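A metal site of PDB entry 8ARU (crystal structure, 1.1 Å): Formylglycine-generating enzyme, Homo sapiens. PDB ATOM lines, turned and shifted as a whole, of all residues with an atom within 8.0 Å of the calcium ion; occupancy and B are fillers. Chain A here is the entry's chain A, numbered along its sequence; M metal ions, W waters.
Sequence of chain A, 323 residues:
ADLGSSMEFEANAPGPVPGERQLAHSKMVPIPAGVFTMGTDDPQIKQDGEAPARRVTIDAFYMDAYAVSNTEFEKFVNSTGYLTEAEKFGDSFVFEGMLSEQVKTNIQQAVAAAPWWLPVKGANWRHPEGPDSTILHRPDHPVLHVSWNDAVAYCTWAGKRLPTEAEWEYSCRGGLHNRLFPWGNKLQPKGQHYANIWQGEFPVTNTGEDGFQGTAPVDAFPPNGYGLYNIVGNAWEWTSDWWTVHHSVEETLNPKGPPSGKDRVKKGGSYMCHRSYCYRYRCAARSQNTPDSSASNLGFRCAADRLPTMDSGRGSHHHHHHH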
ATOM      1  N   HIS A 193      15.290   6.707 -19.369  1.00  0.00           N
ATOM      2  CA  HIS A 193      15.948   5.643 -20.129  1.00  0.00           C
ATOM      3  C   HIS A 193      17.293   6.122 -20.630  1.00  0.00           C
ATOM      4  O   HIS A 193      17.396   7.224 -21.189  1.00  0.00           O
ATOM      5  CB  HIS A 193      15.062   5.147 -21.272  1.00  0.00           C
ATOM      6  CG  HIS A 193      13.949   4.300 -20.787  1.00  0.00           C
ATOM      7  ND1 HIS A 193      14.125   2.977 -20.453  1.00  0.00           N
ATOM      8  CD2 HIS A 193      12.663   4.606 -20.501  1.00  0.00           C
ATOM      9  CE1 HIS A 193      12.987   2.494 -19.971  1.00  0.00           C
ATOM     10  NE2 HIS A 193      12.080   3.452 -20.002  1.00  0.00           N
ATOM     11  N   ALA A 195      19.460   3.769 -22.395  1.00  0.00           N
ATOM     12  CA  ALA A 195      19.866   2.880 -23.489  1.00  0.00           C
ATOM     13  C   ALA A 195      18.634   2.229 -24.085  1.00  0.00           C
ATOM     14  O   ALA A 195      17.584   2.105 -23.427  1.00  0.00           O
ATOM     15  CB  ALA A 195      20.818   1.788 -22.953  1.00  0.00           C
ATOM     16  N   ASN A 196      18.796   1.748 -25.334  1.00  0.00           N
ATOM     17  CA  ASN A 196      17.732   1.092 -26.078  1.00  0.00           C
ATOM     18  C   ASN A 196      17.823  -0.417 -25.864  1.00  0.00           C
ATOM     19  O   ASN A 196      18.640  -1.103 -26.505  1.00  0.00           O
ATOM     20  CB  ASN A 196      17.869   1.448 -27.542  1.00  0.00           C
ATOM     21  CG  ASN A 196      16.805   0.785 -28.372  1.00  0.00           C
ATOM     22  OD1 ASN A 196      15.757   0.382 -27.831  1.00  0.00           O
ATOM     23  ND2 ASN A 196      17.029   0.695 -29.674  1.00  0.00           N
ATOM     24  N   ILE A 197      16.987  -0.935 -24.962  1.00  0.00           N
ATOM     25  CA  ILE A 197      16.847  -2.372 -24.717  1.00  0.00           C
ATOM     26  C   ILE A 197      15.377  -2.730 -24.834  1.00  0.00           C
ATOM     27  O   ILE A 197      14.618  -1.969 -25.413  1.00  0.00           O
ATOM     28  CB  ILE A 197      17.516  -2.818 -23.413  1.00  0.00           C
ATOM     29  CG1 ILE A 197      16.929  -2.115 -22.166  1.00  0.00           C
ATOM     30  CG2 ILE A 197      19.040  -2.579 -23.546  1.00  0.00           C
ATOM     31  CD1 ILE A 197      17.430  -2.736 -20.879  1.00  0.00           C
ATOM     32  N   TRP A 198      14.952  -3.879 -24.316  1.00  0.00           N
ATOM     33  CA  TRP A 198      13.564  -4.328 -24.446  1.00  0.00           C
ATOM     34  C   TRP A 198      12.818  -3.966 -23.166  1.00  0.00           C
ATOM     35  O   TRP A 198      13.356  -4.117 -22.065  1.00  0.00           O
ATOM     36  CB  TRP A 198      13.592  -5.847 -24.537  1.00  0.00           C
ATOM     37  CG  TRP A 198      12.305  -6.529 -24.820  1.00  0.00           C
ATOM     38  CD1 TRP A 198      11.283  -6.807 -23.952  1.00  0.00           C
ATOM     39  CD2 TRP A 198      11.866  -7.016 -26.101  1.00  0.00           C
ATOM     40  NE1 TRP A 198      10.274  -7.485 -24.600  1.00  0.00           N
ATOM     41  CE2 TRP A 198      10.597  -7.626 -25.931  1.00  0.00           C
ATOM     42  CE3 TRP A 198      12.450  -7.039 -27.381  1.00  0.00           C
ATOM     43  CZ2 TRP A 198       9.896  -8.259 -26.988  1.00  0.00           C
ATOM     44  CZ3 TRP A 198      11.756  -7.660 -28.438  1.00  0.00           C
ATOM     45  CH2 TRP A 198      10.496  -8.259 -28.227  1.00  0.00           C
ATOM     46  N   GLN A 199      11.577  -3.534 -23.296  1.00  0.00           N
ATOM     47  CA  GLN A 199      10.643  -3.494 -22.173  1.00  0.00           C
ATOM     48  C   GLN A 199       9.439  -4.338 -22.546  1.00  0.00           C
ATOM     49  O   GLN A 199       9.006  -4.328 -23.703  1.00  0.00           O
ATOM     50  CB  GLN A 199      10.201  -2.074 -21.816  1.00  0.00           C
ATOM     51  CG  GLN A 199      11.312  -1.152 -21.358  1.00  0.00           C
ATOM     52  CD  GLN A 199      12.060  -0.528 -22.546  1.00  0.00           C
ATOM     53  OE1 GLN A 199      11.412  -0.114 -23.522  1.00  0.00           O
ATOM     54  NE2 GLN A 199      13.371  -0.429 -22.462  1.00  0.00           N
ATOM     55  N   ASN A 206       7.171  -6.078 -27.045  1.00  0.00           N
ATOM     56  CA  ASN A 206       8.110  -5.015 -26.766  1.00  0.00           C
ATOM     57  C   ASN A 206       7.271  -3.743 -26.706  1.00  0.00           C
ATOM     58  O   ASN A 206       6.682  -3.343 -27.712  1.00  0.00           O
ATOM     59  CB  ASN A 206       9.153  -4.904 -27.878  1.00  0.00           C
ATOM     60  CG  ASN A 206      10.251  -3.918 -27.538  1.00  0.00           C
ATOM     61  OD1 ASN A 206      10.156  -3.132 -26.575  1.00  0.00           O
ATOM     62  ND2 ASN A 206      11.292  -3.922 -28.322  1.00  0.00           N
ATOM     63  N   THR A 207       7.207  -3.129 -25.523  1.00  0.00           N
ATOM     64  CA  THR A 207       6.330  -1.973 -25.386  1.00  0.00           C
ATOM     65  C   THR A 207       6.883  -0.714 -26.031  1.00  0.00           C
ATOM     66  O   THR A 207       6.126   0.241 -26.247  1.00  0.00           O
ATOM     67  CB  THR A 207       6.060  -1.646 -23.920  1.00  0.00           C
ATOM     68  OG1 THR A 207       7.291  -1.234 -23.331  1.00  0.00           O
ATOM     69  CG2 THR A 207       5.449  -2.861 -23.205  1.00  0.00           C
ATOM     70  N   GLY A 208       8.182  -0.683 -26.322  1.00  0.00           N
ATOM     71  CA  GLY A 208       8.713   0.555 -26.861  1.00  0.00           C
ATOM     72  C   GLY A 208       8.765   1.701 -25.882  1.00  0.00           C
ATOM     73  O   GLY A 208       8.822   2.865 -26.292  1.00  0.00           O
ATOM     74  N   GLU A 209       8.757   1.392 -24.585  1.00  0.00           N
ATOM     75  CA  GLU A 209       8.712   2.430 -23.560  1.00  0.00           C
ATOM     76  C   GLU A 209       9.907   3.365 -23.679  1.00  0.00           C
ATOM     77  O   GLU A 209       9.771   4.563 -23.439  1.00  0.00           O
ATOM     78  CB  GLU A 209       8.710   1.750 -22.195  1.00  0.00           C
ATOM     79  CG  GLU A 209       8.696   2.698 -21.017  1.00  0.00           C
ATOM     80  CD  GLU A 209       9.058   1.974 -19.727  1.00  0.00           C
ATOM     81  OE1 GLU A 209       8.743   0.765 -19.593  1.00  0.00           O
ATOM     82  OE2 GLU A 209       9.592   2.648 -18.824  1.00  0.00           O
ATOM     83  N   ASP A 210      11.086   2.845 -24.066  1.00  0.00           N
ATOM     84  CA  ASP A 210      12.275   3.695 -24.171  1.00  0.00           C
ATOM     85  C   ASP A 210      12.310   4.531 -25.454  1.00  0.00           C
ATOM     86  O   ASP A 210      13.293   5.250 -25.682  1.00  0.00           O
ATOM     87  CB  ASP A 210      13.547   2.863 -23.972  1.00  0.00           C
ATOM     88  CG  ASP A 210      13.740   1.806 -25.052  1.00  0.00           C
ATOM     89  OD1 ASP A 210      13.148   1.929 -26.143  1.00  0.00           O
ATOM     90  OD2 ASP A 210      14.500   0.858 -24.799  1.00  0.00           O
ATOM     91  N   GLY A 211      11.283   4.439 -26.303  1.00  0.00           N
ATOM     92  CA  GLY A 211      11.201   5.208 -27.517  1.00  0.00           C
ATOM     93  C   GLY A 211      11.501   4.440 -28.787  1.00  0.00           C
ATOM     94  O   GLY A 211      11.308   5.018 -29.861  1.00  0.00           O
ATOM     95  N   PHE A 212      11.973   3.189 -28.703  1.00  0.00           N
ATOM     96  CA  PHE A 212      12.422   2.462 -29.898  1.00  0.00           C
ATOM     97  C   PHE A 212      12.133   0.969 -29.736  1.00  0.00           C
ATOM     98  O   PHE A 212      12.588   0.360 -28.761  1.00  0.00           O
ATOM     99  CB  PHE A 212      13.927   2.680 -30.162  1.00  0.00           C
ATOM    100  CG  PHE A 212      14.273   4.120 -30.317  1.00  0.00           C
ATOM    101  CD1 PHE A 212      14.137   4.758 -31.549  1.00  0.00           C
ATOM    102  CD2 PHE A 212      14.643   4.876 -29.176  1.00  0.00           C
ATOM    103  CE1 PHE A 212      14.363   6.133 -31.676  1.00  0.00           C
ATOM    104  CE2 PHE A 212      14.887   6.249 -29.290  1.00  0.00           C
ATOM    105  CZ  PHE A 212      14.701   6.889 -30.544  1.00  0.00           C
ATOM    106  N   GLN A 213      11.357   0.428 -30.662  1.00  0.00           N
ATOM    107  CA  GLN A 213      11.153  -1.002 -30.803  1.00  0.00           C
ATOM    108  C   GLN A 213      12.427  -1.689 -31.320  1.00  0.00           C
ATOM    109  O   GLN A 213      13.068  -2.462 -30.603  1.00  0.00           O
ATOM    110  CB  GLN A 213       9.967  -1.257 -31.743  1.00  0.00           C
ATOM    111  CG  GLN A 213       8.617  -0.883 -31.121  1.00  0.00           C
ATOM    112  CD  GLN A 213       8.073  -1.967 -30.228  1.00  0.00           C
ATOM    113  OE1 GLN A 213       8.548  -3.098 -30.271  1.00  0.00           O
ATOM    114  NE2 GLN A 213       7.070  -1.649 -29.412  1.00  0.00           N
ATOM    115  N   GLY A 214      12.815  -1.371 -32.561  1.00  0.00           N
ATOM    116  CA  GLY A 214      14.049  -1.829 -33.171  1.00  0.00           C
ATOM    117  C   GLY A 214      15.166  -0.900 -32.749  1.00  0.00           C
ATOM    118  O   GLY A 214      15.197  -0.383 -31.619  1.00  0.00           O
ATOM    119  N   THR A 215      16.129  -0.687 -33.635  1.00  0.00           N
ATOM    120  CA  THR A 215      17.243   0.204 -33.315  1.00  0.00           C
ATOM    121  C   THR A 215      16.782   1.645 -33.192  1.00  0.00           C
ATOM    122  O   THR A 215      15.716   2.046 -33.670  1.00  0.00           O
ATOM    123  CB  THR A 215      18.309   0.143 -34.441  1.00  0.00           C
ATOM    124  OG1 THR A 215      17.715   0.462 -35.713  1.00  0.00           O
ATOM    125  CG2 THR A 215      18.967  -1.235 -34.463  1.00  0.00           C
ATOM    126  N   ALA A 216      17.642   2.433 -32.583  1.00  0.00           N
ATOM    127  CA  ALA A 216      17.543   3.877 -32.503  1.00  0.00           C
ATOM    128  C   ALA A 216      18.658   4.513 -33.317  1.00  0.00           C
ATOM    129  O   ALA A 216      19.692   3.875 -33.562  1.00  0.00           O
ATOM    130  CB  ALA A 216      17.696   4.304 -31.045  1.00  0.00           C
ATOM    131  N   PHE A 221      20.002   8.850 -26.964  1.00  0.00           N
ATOM    132  CA  PHE A 221      20.281   8.590 -25.537  1.00  0.00           C
ATOM    133  C   PHE A 221      21.466   9.394 -25.050  1.00  0.00           C
ATOM    134  O   PHE A 221      22.225   9.959 -25.845  1.00  0.00           O
ATOM    135  CB  PHE A 221      20.365   7.076 -25.213  1.00  0.00           C
ATOM    136  CG  PHE A 221      19.047   6.377 -25.449  1.00  0.00           C
ATOM    137  CD1 PHE A 221      18.012   6.456 -24.510  1.00  0.00           C
ATOM    138  CD2 PHE A 221      18.817   5.661 -26.634  1.00  0.00           C
ATOM    139  CE1 PHE A 221      16.778   5.826 -24.775  1.00  0.00           C
ATOM    140  CE2 PHE A 221      17.585   5.085 -26.904  1.00  0.00           C
ATOM    141  CZ  PHE A 221      16.560   5.159 -25.956  1.00  0.00           C
ATOM    142  N   ASN A 234      21.026  -1.078 -28.078  1.00  0.00           N
ATOM    143  CA  ASN A 234      20.905  -0.701 -29.487  1.00  0.00           C
ATOM    144  C   ASN A 234      21.277  -1.878 -30.391  1.00  0.00           C
ATOM    145  O   ASN A 234      20.374  -2.565 -30.888  1.00  0.00           O
ATOM    146  CB  ASN A 234      21.578   0.636 -29.849  1.00  0.00           C
ATOM    147  CG  ASN A 234      20.773   1.419 -30.883  1.00  0.00           C
ATOM    148  OD1 ASN A 234      19.562   1.222 -31.003  1.00  0.00           O
ATOM    149  ND2 ASN A 234      21.427   2.286 -31.664  1.00  0.00           N
ATOM    150  N   SER A 270      21.838  -5.419 -27.093  1.00  0.00           N
ATOM    151  CA  SER A 270      21.069  -4.861 -28.190  1.00  0.00           C
ATOM    152  C   SER A 270      19.680  -4.424 -27.729  1.00  0.00           C
ATOM    153  O   SER A 270      19.291  -4.613 -26.570  1.00  0.00           O
ATOM    154  CB  SER A 270      20.926  -5.846 -29.361  1.00  0.00           C
ATOM    155  OG  SER A 270      19.943  -6.822 -29.059  1.00  0.00           O
ATOM    156  N   TYR A 271      18.910  -3.907 -28.698  1.00  0.00           N
ATOM    157  CA  TYR A 271      17.519  -3.546 -28.466  1.00  0.00           C
ATOM    158  C   TYR A 271      16.631  -4.716 -28.044  1.00  0.00           C
ATOM    159  O   TYR A 271      15.515  -4.478 -27.542  1.00  0.00           O
ATOM    160  CB  TYR A 271      16.928  -2.870 -29.720  1.00  0.00           C
ATOM    161  CG  TYR A 271      16.671  -3.788 -30.917  1.00  0.00           C
ATOM    162  CD1 TYR A 271      15.529  -4.573 -30.977  1.00  0.00           C
ATOM    163  CD2 TYR A 271      17.576  -3.853 -31.988  1.00  0.00           C
ATOM    164  CE1 TYR A 271      15.246  -5.383 -32.053  1.00  0.00           C
ATOM    165  CE2 TYR A 271      17.311  -4.641 -33.096  1.00  0.00           C
ATOM    166  CZ  TYR A 271      16.139  -5.394 -33.125  1.00  0.00           C
ATOM    167  OH  TYR A 271      15.809  -6.180 -34.203  1.00  0.00           O
ATOM    168  N   MET A 272      17.110  -5.951 -28.213  1.00  0.00           N
ATOM    169  CA  MET A 272      16.384  -7.149 -27.821  1.00  0.00           C
ATOM    170  C   MET A 272      16.526  -7.506 -26.354  1.00  0.00           C
ATOM    171  O   MET A 272      15.787  -8.372 -25.846  1.00  0.00           O
ATOM    172  CB  MET A 272      16.831  -8.350 -28.641  1.00  0.00           C
ATOM    173  CG  MET A 272      16.549  -8.199 -30.107  1.00  0.00           C
ATOM    174  SD  MET A 272      17.280  -9.506 -31.099  1.00  0.00           S
ATOM    175  CE  MET A 272      16.493 -10.978 -30.479  1.00  0.00           C
ATOM    176  N   CYS A 273      17.495  -6.936 -25.633  1.00  0.00           N
ATOM    177  CA  CYS A 273      17.860  -7.533 -24.385  1.00  0.00           C
ATOM    178  C   CYS A 273      16.914  -7.129 -23.244  1.00  0.00           C
ATOM    179  O   CYS A 273      16.529  -5.982 -23.132  1.00  0.00           O
ATOM    180  CB  CYS A 273      19.292  -7.158 -24.073  1.00  0.00           C
ATOM    181  SG  CYS A 273      19.917  -8.091 -22.784  1.00  0.00           S
HETATM  182 CA    CA M   1      13.807  -0.332 -26.870  1.00  0.00          CA
HETATM  183  O   HOH W   1      11.656  -0.970 -26.072  1.00  0.00           O
HETATM  184  O   HOH W   2      13.786  -2.343 -28.148  1.00  0.00           O
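OD1 of Asn 196 is bound to the calcium ion, at 2.3 Å.
The backbone carbonyl oxygen (O) of Ile 197 is bound to the calcium ion, at 2.3 Å.
The backbone carbonyl oxygen (O) of Phe 212 is bound to the calcium ion (2.4 Å).
The calcium ion is bound by water W1 (2.4 Å).
The calcium ion is bound by water W2, at 2.4 Å.
The calcium ion is bound by the side-chain carboxylate (OD1) of Asp 210 (2.5 Å).
OD2 of Asp 210 is bound to the calcium ion, 2.5 Å away.
Water W2 lies within hydrogen-bond range of O of Gln 213 (2.6 Å), O of Tyr 271 (2.8 Å) and ND2 of Asn 206 (3.0 Å).
Water W1 lies within hydrogen-bond range of the side-chain amide oxygen of Asn 206, the side-chain amide oxygen of Gln 199 and the backbone NH of Gly 208.
The nearest printed residue that does not touch the calcium ion is Gln 199 (4.1 Å).
N of Asn 234 lies within hydrogen-bond range of O of Asn 196, 2.9 Å away.
O of Gly 214 lies within hydrogen-bond range of ND2 of Asn 196 (2.9 Å).
The backbone NH of Ala 216 sits close to the side-chain amide nitrogen of Asn 196 (3.4 Å).
The backbone NH of Asp 210 is in hydrogen-bond range of the side-chain amide oxygen of Gln 199, 3.0 Å away.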
